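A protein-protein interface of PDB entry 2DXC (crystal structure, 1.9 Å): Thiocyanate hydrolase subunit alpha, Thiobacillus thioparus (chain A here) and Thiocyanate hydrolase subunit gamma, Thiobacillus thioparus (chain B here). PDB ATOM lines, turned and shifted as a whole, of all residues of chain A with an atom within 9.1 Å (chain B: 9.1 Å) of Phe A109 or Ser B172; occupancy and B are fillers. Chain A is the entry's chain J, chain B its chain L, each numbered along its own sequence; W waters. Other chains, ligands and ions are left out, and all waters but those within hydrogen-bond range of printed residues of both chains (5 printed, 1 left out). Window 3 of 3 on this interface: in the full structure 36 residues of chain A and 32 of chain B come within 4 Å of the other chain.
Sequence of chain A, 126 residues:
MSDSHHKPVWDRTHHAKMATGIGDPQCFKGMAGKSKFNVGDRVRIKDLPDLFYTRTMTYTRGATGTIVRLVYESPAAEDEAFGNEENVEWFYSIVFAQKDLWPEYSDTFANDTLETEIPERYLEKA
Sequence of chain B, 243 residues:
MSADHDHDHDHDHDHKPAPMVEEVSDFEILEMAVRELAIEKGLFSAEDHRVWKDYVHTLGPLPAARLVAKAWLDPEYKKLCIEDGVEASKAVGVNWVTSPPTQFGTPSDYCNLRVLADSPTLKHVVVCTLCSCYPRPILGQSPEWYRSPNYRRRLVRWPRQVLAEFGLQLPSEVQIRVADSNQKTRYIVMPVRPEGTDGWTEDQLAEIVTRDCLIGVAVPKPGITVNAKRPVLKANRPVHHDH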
ATOM      1  N   ALA A  97     -19.551  22.349  16.325  1.00  0.00           N
ATOM      2  CA  ALA A  97     -18.240  22.985  16.276  1.00  0.00           C
ATOM      3  C   ALA A  97     -17.728  22.810  17.706  1.00  0.00           C
ATOM      4  O   ALA A  97     -18.456  23.089  18.656  1.00  0.00           O
ATOM      5  CB  ALA A  97     -18.376  24.463  15.939  1.00  0.00           C
ATOM      6  N   GLN A  98     -16.496  22.335  17.867  1.00  0.00           N
ATOM      7  CA  GLN A  98     -15.944  22.116  19.204  1.00  0.00           C
ATOM      8  C   GLN A  98     -16.026  23.366  20.080  1.00  0.00           C
ATOM      9  O   GLN A  98     -16.260  23.274  21.284  1.00  0.00           O
ATOM     10  CB  GLN A  98     -14.492  21.628  19.107  1.00  0.00           C
ATOM     11  CG  GLN A  98     -14.357  20.178  18.626  1.00  0.00           C
ATOM     12  CD  GLN A  98     -14.727  19.168  19.699  1.00  0.00           C
ATOM     13  OE1 GLN A  98     -15.737  19.315  20.392  1.00  0.00           O
ATOM     14  NE2 GLN A  98     -13.909  18.132  19.841  1.00  0.00           N
ATOM     15  N   LYS A  99     -15.850  24.533  19.469  1.00  0.00           N
ATOM     16  CA  LYS A  99     -15.916  25.792  20.205  1.00  0.00           C
ATOM     17  C   LYS A  99     -17.283  25.995  20.856  1.00  0.00           C
ATOM     18  O   LYS A  99     -17.392  26.696  21.858  1.00  0.00           O
ATOM     19  CB  LYS A  99     -15.612  26.970  19.273  1.00  0.00           C
ATOM     20  CG  LYS A  99     -16.541  27.044  18.068  1.00  0.00           C
ATOM     21  CD  LYS A  99     -16.171  28.168  17.098  1.00  0.00           C
ATOM     22  CE  LYS A  99     -16.555  29.545  17.629  1.00  0.00           C
ATOM     23  NZ  LYS A  99     -15.778  29.938  18.840  1.00  0.00           N
ATOM     24  N   ASP A 100     -18.325  25.389  20.295  1.00  0.00           N
ATOM     25  CA  ASP A 100     -19.663  25.551  20.862  1.00  0.00           C
ATOM     26  C   ASP A 100     -19.972  24.577  21.997  1.00  0.00           C
ATOM     27  O   ASP A 100     -20.999  24.695  22.662  1.00  0.00           O
ATOM     28  CB  ASP A 100     -20.731  25.435  19.767  1.00  0.00           C
ATOM     29  CG  ASP A 100     -20.632  26.551  18.733  1.00  0.00           C
ATOM     30  OD1 ASP A 100     -20.256  27.679  19.112  1.00  0.00           O
ATOM     31  OD2 ASP A 100     -20.943  26.303  17.549  1.00  0.00           O
ATOM     32  N   GLU A 104     -13.328  26.585  26.573  1.00  0.00           N
ATOM     33  CA  GLU A 104     -11.884  26.752  26.469  1.00  0.00           C
ATOM     34  C   GLU A 104     -11.237  26.307  25.159  1.00  0.00           C
ATOM     35  O   GLU A 104     -10.027  26.475  24.985  1.00  0.00           O
ATOM     36  CB  GLU A 104     -11.188  26.024  27.631  1.00  0.00           C
ATOM     37  CG  GLU A 104     -11.002  24.503  27.455  1.00  0.00           C
ATOM     38  CD  GLU A 104     -12.295  23.694  27.593  1.00  0.00           C
ATOM     39  OE1 GLU A 104     -13.340  24.269  27.960  1.00  0.00           O
ATOM     40  OE2 GLU A 104     -12.256  22.470  27.343  1.00  0.00           O
ATOM     41  N   TYR A 105     -12.014  25.743  24.238  1.00  0.00           N
ATOM     42  CA  TYR A 105     -11.424  25.282  22.985  1.00  0.00           C
ATOM     43  C   TYR A 105     -10.690  26.419  22.279  1.00  0.00           C
ATOM     44  O   TYR A 105     -11.220  27.519  22.131  1.00  0.00           O
ATOM     45  CB  TYR A 105     -12.487  24.684  22.058  1.00  0.00           C
ATOM     46  CG  TYR A 105     -11.954  23.504  21.278  1.00  0.00           C
ATOM     47  CD1 TYR A 105     -11.768  22.267  21.897  1.00  0.00           C
ATOM     48  CD2 TYR A 105     -11.577  23.636  19.941  1.00  0.00           C
ATOM     49  CE1 TYR A 105     -11.220  21.186  21.206  1.00  0.00           C
ATOM     50  CE2 TYR A 105     -11.024  22.560  19.236  1.00  0.00           C
ATOM     51  CZ  TYR A 105     -10.848  21.340  19.876  1.00  0.00           C
ATOM     52  OH  TYR A 105     -10.292  20.282  19.194  1.00  0.00           O
ATOM     53  N   SER A 106      -9.468  26.143  21.837  1.00  0.00           N
ATOM     54  CA  SER A 106      -8.640  27.154  21.184  1.00  0.00           C
ATOM     55  C   SER A 106      -9.038  27.522  19.759  1.00  0.00           C
ATOM     56  O   SER A 106      -9.379  26.654  18.957  1.00  0.00           O
ATOM     57  CB  SER A 106      -7.176  26.703  21.191  1.00  0.00           C
ATOM     58  OG  SER A 106      -6.363  27.620  20.480  1.00  0.00           O
ATOM     59  N   ASP A 107      -8.981  28.817  19.451  1.00  0.00           N
ATOM     60  CA  ASP A 107      -9.304  29.301  18.115  1.00  0.00           C
ATOM     61  C   ASP A 107      -8.248  28.828  17.121  1.00  0.00           C
ATOM     62  O   ASP A 107      -8.439  28.943  15.913  1.00  0.00           O
ATOM     63  CB  ASP A 107      -9.362  30.832  18.078  1.00  0.00           C
ATOM     64  CG  ASP A 107     -10.534  31.394  18.853  1.00  0.00           C
ATOM     65  OD1 ASP A 107     -11.649  30.838  18.740  1.00  0.00           O
ATOM     66  OD2 ASP A 107     -10.341  32.402  19.564  1.00  0.00           O
ATOM     67  N   THR A 108      -7.132  28.314  17.633  1.00  0.00           N
ATOM     68  CA  THR A 108      -6.063  27.812  16.775  1.00  0.00           C
ATOM     69  C   THR A 108      -6.579  26.595  16.015  1.00  0.00           C
ATOM     70  O   THR A 108      -6.204  26.357  14.866  1.00  0.00           O
ATOM     71  CB  THR A 108      -4.813  27.407  17.597  1.00  0.00           C
ATOM     72  OG1 THR A 108      -4.219  28.576  18.176  1.00  0.00           O
ATOM     73  CG2 THR A 108      -3.780  26.719  16.709  1.00  0.00           C
ATOM     74  N   PHE A 109      -7.442  25.825  16.669  1.00  0.00           N
ATOM     75  CA  PHE A 109      -8.034  24.638  16.063  1.00  0.00           C
ATOM     76  C   PHE A 109      -9.490  24.977  15.759  1.00  0.00           C
ATOM     77  O   PHE A 109     -10.409  24.253  16.132  1.00  0.00           O
ATOM     78  CB  PHE A 109      -7.932  23.472  17.038  1.00  0.00           C
ATOM     79  CG  PHE A 109      -6.544  23.266  17.566  1.00  0.00           C
ATOM     80  CD1 PHE A 109      -5.501  22.939  16.702  1.00  0.00           C
ATOM     81  CD2 PHE A 109      -6.269  23.433  18.919  1.00  0.00           C
ATOM     82  CE1 PHE A 109      -4.203  22.780  17.177  1.00  0.00           C
ATOM     83  CE2 PHE A 109      -4.973  23.278  19.406  1.00  0.00           C
ATOM     84  CZ  PHE A 109      -3.938  22.951  18.532  1.00  0.00           C
ATOM     85  N   ALA A 110      -9.671  26.095  15.066  1.00  0.00           N
ATOM     86  CA  ALA A 110     -10.986  26.617  14.713  1.00  0.00           C
ATOM     87  C   ALA A 110     -11.898  25.713  13.892  1.00  0.00           C
ATOM     88  O   ALA A 110     -13.110  25.922  13.874  1.00  0.00           O
ATOM     89  CB  ALA A 110     -10.821  27.950  13.997  1.00  0.00           C
ATOM     90  N   ASN A 111     -11.334  24.713  13.219  1.00  0.00           N
ATOM     91  CA  ASN A 111     -12.148  23.828  12.391  1.00  0.00           C
ATOM     92  C   ASN A 111     -12.558  22.491  13.011  1.00  0.00           C
ATOM     93  O   ASN A 111     -13.275  21.712  12.382  1.00  0.00           O
ATOM     94  CB  ASN A 111     -11.434  23.565  11.061  1.00  0.00           C
ATOM     95  CG  ASN A 111     -11.216  24.835  10.259  1.00  0.00           C
ATOM     96  OD1 ASN A 111     -12.128  25.645  10.106  1.00  0.00           O
ATOM     97  ND2 ASN A 111     -10.009  25.011   9.737  1.00  0.00           N
ATOM     98  N   ASP A 112     -12.124  22.217  14.236  1.00  0.00           N
ATOM     99  CA  ASP A 112     -12.459  20.943  14.867  1.00  0.00           C
ATOM    100  C   ASP A 112     -13.945  20.781  15.165  1.00  0.00           C
ATOM    101  O   ASP A 112     -14.631  21.742  15.518  1.00  0.00           O
ATOM    102  CB  ASP A 112     -11.638  20.753  16.142  1.00  0.00           C
ATOM    103  CG  ASP A 112     -10.158  20.577  15.856  1.00  0.00           C
ATOM    104  OD1 ASP A 112      -9.773  20.529  14.663  1.00  0.00           O
ATOM    105  OD2 ASP A 112      -9.377  20.480  16.826  1.00  0.00           O
ATOM    106  N   THR A 113     -14.432  19.551  15.034  1.00  0.00           N
ATOM    107  CA  THR A 113     -15.840  19.264  15.256  1.00  0.00           C
ATOM    108  C   THR A 113     -16.081  17.938  15.966  1.00  0.00           C
ATOM    109  O   THR A 113     -15.158  17.152  16.194  1.00  0.00           O
ATOM    110  CB  THR A 113     -16.593  19.200  13.923  1.00  0.00           C
ATOM    111  OG1 THR A 113     -15.976  18.214  13.084  1.00  0.00           O
ATOM    112  CG2 THR A 113     -16.555  20.541  13.214  1.00  0.00           C
ATOM    113  N   PRO B 120      -7.304  15.534   3.029  1.00  0.00           N
ATOM    114  CA  PRO B 120      -6.237  16.465   3.402  1.00  0.00           C
ATOM    115  C   PRO B 120      -6.701  17.535   4.402  1.00  0.00           C
ATOM    116  O   PRO B 120      -5.878  18.177   5.052  1.00  0.00           O
ATOM    117  CB  PRO B 120      -5.822  17.065   2.060  1.00  0.00           C
ATOM    118  CG  PRO B 120      -6.027  15.909   1.114  1.00  0.00           C
ATOM    119  CD  PRO B 120      -7.374  15.373   1.563  1.00  0.00           C
ATOM    120  N   THR B 121      -8.012  17.715   4.528  1.00  0.00           N
ATOM    121  CA  THR B 121      -8.560  18.721   5.442  1.00  0.00           C
ATOM    122  C   THR B 121      -9.465  18.150   6.538  1.00  0.00           C
ATOM    123  O   THR B 121     -10.114  18.910   7.259  1.00  0.00           O
ATOM    124  CB  THR B 121      -9.386  19.770   4.673  1.00  0.00           C
ATOM    125  OG1 THR B 121     -10.485  19.120   4.022  1.00  0.00           O
ATOM    126  CG2 THR B 121      -8.527  20.476   3.631  1.00  0.00           C
ATOM    127  N   ARG B 157     -13.434  16.048  24.237  1.00  0.00           N
ATOM    128  CA  ARG B 157     -13.110  17.409  24.651  1.00  0.00           C
ATOM    129  C   ARG B 157     -11.681  17.876  24.373  1.00  0.00           C
ATOM    130  O   ARG B 157     -11.448  19.050  24.064  1.00  0.00           O
ATOM    131  CB  ARG B 157     -13.415  17.557  26.144  1.00  0.00           C
ATOM    132  CG  ARG B 157     -13.222  18.952  26.688  1.00  0.00           C
ATOM    133  CD  ARG B 157     -13.905  19.091  28.035  1.00  0.00           C
ATOM    134  NE  ARG B 157     -14.071  20.491  28.414  1.00  0.00           N
ATOM    135  CZ  ARG B 157     -14.856  20.913  29.397  1.00  0.00           C
ATOM    136  NH1 ARG B 157     -15.559  20.045  30.118  1.00  0.00           N
ATOM    137  NH2 ARG B 157     -14.953  22.211  29.644  1.00  0.00           N
ATOM    138  N   TRP B 158     -10.725  16.961  24.491  1.00  0.00           N
ATOM    139  CA  TRP B 158      -9.324  17.289  24.255  1.00  0.00           C
ATOM    140  C   TRP B 158      -8.743  16.303  23.235  1.00  0.00           C
ATOM    141  O   TRP B 158      -7.742  15.640  23.503  1.00  0.00           O
ATOM    142  CB  TRP B 158      -8.552  17.195  25.580  1.00  0.00           C
ATOM    143  CG  TRP B 158      -9.033  18.151  26.654  1.00  0.00           C
ATOM    144  CD1 TRP B 158      -8.783  19.494  26.732  1.00  0.00           C
ATOM    145  CD2 TRP B 158      -9.853  17.832  27.790  1.00  0.00           C
ATOM    146  NE1 TRP B 158      -9.393  20.029  27.845  1.00  0.00           N
ATOM    147  CE2 TRP B 158     -10.056  19.032  28.511  1.00  0.00           C
ATOM    148  CE3 TRP B 158     -10.434  16.651  28.267  1.00  0.00           C
ATOM    149  CZ2 TRP B 158     -10.818  19.083  29.685  1.00  0.00           C
ATOM    150  CZ3 TRP B 158     -11.195  16.703  29.440  1.00  0.00           C
ATOM    151  CH2 TRP B 158     -11.377  17.912  30.132  1.00  0.00           C
ATOM    152  N   PRO B 159      -9.359  16.205  22.044  1.00  0.00           N
ATOM    153  CA  PRO B 159      -8.866  15.273  21.021  1.00  0.00           C
ATOM    154  C   PRO B 159      -7.422  15.485  20.571  1.00  0.00           C
ATOM    155  O   PRO B 159      -6.676  14.521  20.398  1.00  0.00           O
ATOM    156  CB  PRO B 159      -9.872  15.441  19.885  1.00  0.00           C
ATOM    157  CG  PRO B 159     -10.307  16.866  20.020  1.00  0.00           C
ATOM    158  CD  PRO B 159     -10.471  17.021  21.518  1.00  0.00           C
ATOM    159  N   ARG B 160      -7.033  16.741  20.383  1.00  0.00           N
ATOM    160  CA  ARG B 160      -5.670  17.064  19.964  1.00  0.00           C
ATOM    161  C   ARG B 160      -4.676  16.540  20.999  1.00  0.00           C
ATOM    162  O   ARG B 160      -3.651  15.947  20.657  1.00  0.00           O
ATOM    163  CB  ARG B 160      -5.511  18.581  19.834  1.00  0.00           C
ATOM    164  CG  ARG B 160      -6.396  19.214  18.773  1.00  0.00           C
ATOM    165  CD  ARG B 160      -5.704  19.231  17.434  1.00  0.00           C
ATOM    166  NE  ARG B 160      -6.543  19.773  16.368  1.00  0.00           N
ATOM    167  CZ  ARG B 160      -6.103  20.001  15.134  1.00  0.00           C
ATOM    168  NH1 ARG B 160      -4.836  19.735  14.833  1.00  0.00           N
ATOM    169  NH2 ARG B 160      -6.921  20.475  14.202  1.00  0.00           N
ATOM    170  N   GLN B 161      -4.994  16.760  22.269  1.00  0.00           N
ATOM    171  CA  GLN B 161      -4.126  16.326  23.356  1.00  0.00           C
ATOM    172  C   GLN B 161      -4.061  14.802  23.476  1.00  0.00           C
ATOM    173  O   GLN B 161      -2.976  14.228  23.593  1.00  0.00           O
ATOM    174  CB  GLN B 161      -4.588  16.953  24.678  1.00  0.00           C
ATOM    175  CG  GLN B 161      -4.467  18.483  24.717  1.00  0.00           C
ATOM    176  CD  GLN B 161      -5.585  19.205  23.978  1.00  0.00           C
ATOM    177  OE1 GLN B 161      -6.464  18.580  23.383  1.00  0.00           O
ATOM    178  NE2 GLN B 161      -5.555  20.531  24.017  1.00  0.00           N
ATOM    179  N   GLN B 169      -0.304  13.726  15.419  1.00  0.00           N
ATOM    180  CA  GLN B 169      -0.532  15.161  15.386  1.00  0.00           C
ATOM    181  C   GLN B 169      -0.867  15.592  13.962  1.00  0.00           C
ATOM    182  O   GLN B 169      -0.268  15.107  13.001  1.00  0.00           O
ATOM    183  CB  GLN B 169       0.710  15.907  15.884  1.00  0.00           C
ATOM    184  CG  GLN B 169       0.543  17.414  15.943  1.00  0.00           C
ATOM    185  CD  GLN B 169       1.742  18.121  16.548  1.00  0.00           C
ATOM    186  OE1 GLN B 169       1.859  18.249  17.772  1.00  0.00           O
ATOM    187  NE2 GLN B 169       2.646  18.578  15.690  1.00  0.00           N
ATOM    188  N   LEU B 170      -1.846  16.482  13.829  1.00  0.00           N
ATOM    189  CA  LEU B 170      -2.247  16.993  12.523  1.00  0.00           C
ATOM    190  C   LEU B 170      -2.155  18.513  12.498  1.00  0.00           C
ATOM    191  O   LEU B 170      -2.173  19.158  13.547  1.00  0.00           O
ATOM    192  CB  LEU B 170      -3.682  16.575  12.185  1.00  0.00           C
ATOM    193  CG  LEU B 170      -3.874  15.128  11.729  1.00  0.00           C
ATOM    194  CD1 LEU B 170      -4.168  14.234  12.918  1.00  0.00           C
ATOM    195  CD2 LEU B 170      -5.010  15.077  10.737  1.00  0.00           C
ATOM    196  N   PRO B 171      -2.044  19.104  11.296  1.00  0.00           N
ATOM    197  CA  PRO B 171      -1.955  20.561  11.179  1.00  0.00           C
ATOM    198  C   PRO B 171      -3.120  21.208  11.924  1.00  0.00           C
ATOM    199  O   PRO B 171      -4.226  20.663  11.953  1.00  0.00           O
ATOM    200  CB  PRO B 171      -2.033  20.789   9.672  1.00  0.00           C
ATOM    201  CG  PRO B 171      -1.347  19.567   9.120  1.00  0.00           C
ATOM    202  CD  PRO B 171      -1.934  18.457   9.975  1.00  0.00           C
ATOM    203  N   SER B 172      -2.873  22.369  12.518  1.00  0.00           N
ATOM    204  CA  SER B 172      -3.903  23.066  13.275  1.00  0.00           C
ATOM    205  C   SER B 172      -5.109  23.449  12.421  1.00  0.00           C
ATOM    206  O   SER B 172      -6.228  23.528  12.929  1.00  0.00           O
ATOM    207  CB  SER B 172      -3.318  24.318  13.941  1.00  0.00           C
ATOM    208  OG  SER B 172      -2.905  25.262  12.971  1.00  0.00           O
ATOM    209  N   GLU B 173      -4.897  23.683  11.128  1.00  0.00           N
ATOM    210  CA  GLU B 173      -6.006  24.059  10.261  1.00  0.00           C
ATOM    211  C   GLU B 173      -6.850  22.857   9.819  1.00  0.00           C
ATOM    212  O   GLU B 173      -7.989  23.020   9.382  1.00  0.00           O
ATOM    213  CB  GLU B 173      -5.501  24.833   9.032  1.00  0.00           C
ATOM    214  CG  GLU B 173      -4.640  24.038   8.056  1.00  0.00           C
ATOM    215  CD  GLU B 173      -3.177  23.928   8.481  1.00  0.00           C
ATOM    216  OE1 GLU B 173      -2.384  23.350   7.703  1.00  0.00           O
ATOM    217  OE2 GLU B 173      -2.821  24.416   9.578  1.00  0.00           O
ATOM    218  N   VAL B 174      -6.296  21.654   9.935  1.00  0.00           N
ATOM    219  CA  VAL B 174      -7.028  20.447   9.558  1.00  0.00           C
ATOM    220  C   VAL B 174      -8.176  20.239  10.539  1.00  0.00           C
ATOM    221  O   VAL B 174      -8.023  20.466  11.737  1.00  0.00           O
ATOM    222  CB  VAL B 174      -6.121  19.188   9.598  1.00  0.00           C
ATOM    223  CG1 VAL B 174      -6.969  17.920   9.480  1.00  0.00           C
ATOM    224  CG2 VAL B 174      -5.112  19.238   8.464  1.00  0.00           C
ATOM    225  N   GLN B 175      -9.324  19.813  10.027  1.00  0.00           N
ATOM    226  CA  GLN B 175     -10.475  19.567  10.885  1.00  0.00           C
ATOM    227  C   GLN B 175     -10.407  18.197  11.539  1.00  0.00           C
ATOM    228  O   GLN B 175     -10.490  17.171  10.862  1.00  0.00           O
ATOM    229  CB  GLN B 175     -11.781  19.660  10.086  1.00  0.00           C
ATOM    230  CG  GLN B 175     -13.016  19.190  10.869  1.00  0.00           C
ATOM    231  CD  GLN B 175     -14.298  19.202  10.039  1.00  0.00           C
ATOM    232  OE1 GLN B 175     -14.295  19.579   8.865  1.00  0.00           O
ATOM    233  NE2 GLN B 175     -15.397  18.786  10.649  1.00  0.00           N
ATOM    234  N   ILE B 176     -10.228  18.171  12.854  1.00  0.00           N
ATOM    235  CA  ILE B 176     -10.225  16.898  13.561  1.00  0.00           C
ATOM    236  C   ILE B 176     -11.686  16.704  13.946  1.00  0.00           C
ATOM    237  O   ILE B 176     -12.285  17.579  14.575  1.00  0.00           O
ATOM    238  CB  ILE B 176      -9.392  16.938  14.858  1.00  0.00           C
ATOM    239  CG1 ILE B 176      -7.913  17.114  14.525  1.00  0.00           C
ATOM    240  CG2 ILE B 176      -9.595  15.651  15.648  1.00  0.00           C
ATOM    241  CD1 ILE B 176      -7.298  15.968  13.708  1.00  0.00           C
HETATM  242  O   HOH W   1     -13.677  25.344  30.461  1.00  0.00           O
HETATM  243  O   HOH W   2     -12.617  17.536  17.273  1.00  0.00           O
HETATM  244  O   HOH W   3      -8.352  19.257  21.084  1.00  0.00           O
HETATM  245  O   HOH W   4      -4.666  27.452  12.908  1.00  0.00           O
HETATM  246  O   HOH W   5     -10.970  21.630  25.102  1.00  0.00           O
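The backbone carbonyl oxygen of Thr A108 sits close to the backbone carbonyl oxygen of Ser B172 (3.4 Å). The side-chain carboxylate of Glu A104 is in salt-bridge range of the guanidinium group of Arg B157 (2.9 Å). The side-chain carboxylate of Asp A112 lies close to the backbone carbonyl oxygen of Val B174 (3.4 Å). N of Thr A113 lies within hydrogen-bond range of O of Ile B176, at 3.0 Å. N of Ile B176 sits at hydrogen-bond distance from OD1 of Asp A112, 3.0 Å away. The guanidinium group of Arg B160 lies within salt-bridge range of the side-chain carboxylate of Asp A112 (2.9 Å). OG1 of Thr A113 is in hydrogen-bond range of NE2 of Gln B175 (2.6 Å). The backbone carbonyl oxygen of Glu B173 is in hydrogen-bond range of the side-chain amide nitrogen of Asn A111 (2.9 Å).
NH1 of Arg B160 is in hydrogen-bond range of O of Pro B171, 3.1 Å away. The guanidinium group (NH2) of Arg B160 is in hydrogen-bond range of the backbone carbonyl oxygen (O) of Val B174 (2.7 Å). O of Asp A112 lies within hydrogen-bond range of N of Gln A98. The side-chain carboxylate of Asp A112 lies within hydrogen-bond range of the side-chain hydroxyl of Tyr A105, at 2.5 Å. NH2 of Arg B160 is in hydrogen-bond range of O of Ser B172, 3.4 Å away. The backbone NH of Gln B175 sits at hydrogen-bond distance from the backbone carbonyl oxygen of Thr B121, 3.0 Å away.
Among the printed residues, pairs that only touch across the chains: Asn A111 with Gln B175, Phe A109 with Arg B160, Tyr A105 with Pro B159, Tyr A105 with Arg B157, Phe A109 with Ser B172, Glu A104 with Trp B158, Gln A98 with Pro B159 and Asp A112 with Gln B175.
Printed residues of chain B within 4 Å of Gln A98: Pro B159. Of the printed residues of chain B, Glu A104 touches Arg B157 and Trp B158. Of the printed residues of chain B, Tyr A105 touches Arg B157 and Pro B159. Of the printed residues of chain B, Thr A108 touches Ser B172. Of chain B, only Arg B160 (3.3 Å) and Ser B172 (3.7 Å) come within 4 Å of Phe A109. Ala A110 touches none of the printed residues of chain B. Of the printed residues of chain B, Asn A111 touches Glu B173 and Gln B175. Of chain B, only Arg B160 (2.9 Å), Val B174 (3.4 Å), Gln B175 (3.9 Å) and Ile B176 (3.0 Å) come within 4 Å of Asp A112. Ser B172 touches just these residues of chain A: Thr A108 (3.4 Å) and Phe A109 (3.7 Å). Printed residues of chain A within 4 Å of Glu B173: Asn A111. Printed residues of chain A within 4 Å of Ile B176: Asp A112 and Thr A113. The nearest printed residue of chain B that does not touch Phe A109 is Gln B161 (5.4 Å). The nearest residue of chain A that does not touch Ser B172 is Ala A110 (4.8 Å).
Hydrophobic or aromatic side chains of chain B that line the printed part of chain A: Trp B158, Pro B159 and Ile B176. Along chain B the printed residues that touch a printed residue of chain A span positions 157 to 176. Of the 14 printed residues of chain A, 8 touch a printed residue of chain B. Among the printed residues, 16 pairs touch across the chains.
Water W5 lies within hydrogen-bond range of OE2 of Glu A104 (2.7 Å) and O of Arg B157 (2.8 Å). Water W2 lies within hydrogen-bond range of the backbone carbonyl oxygen of Ile B176, the backbone carbonyl oxygen of Thr A113 and the side-chain amide nitrogen of Gln A98. Water W4 bridges the backbone carbonyl oxygen (O) of Thr A108 (2.7 Å) and the side-chain hydroxyl (OG) of Ser B172 (2.8 Å). Water W1 lies within hydrogen-bond range of OE1 of Glu A104 (2.7 Å) and NH2 of Arg B157 (3.5 Å). Water W3 lies within hydrogen-bond range of OH of Tyr A105 (2.9 Å), N of Arg B160 (2.9 Å) and OE1 of Gln B161 (3.1 Å).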
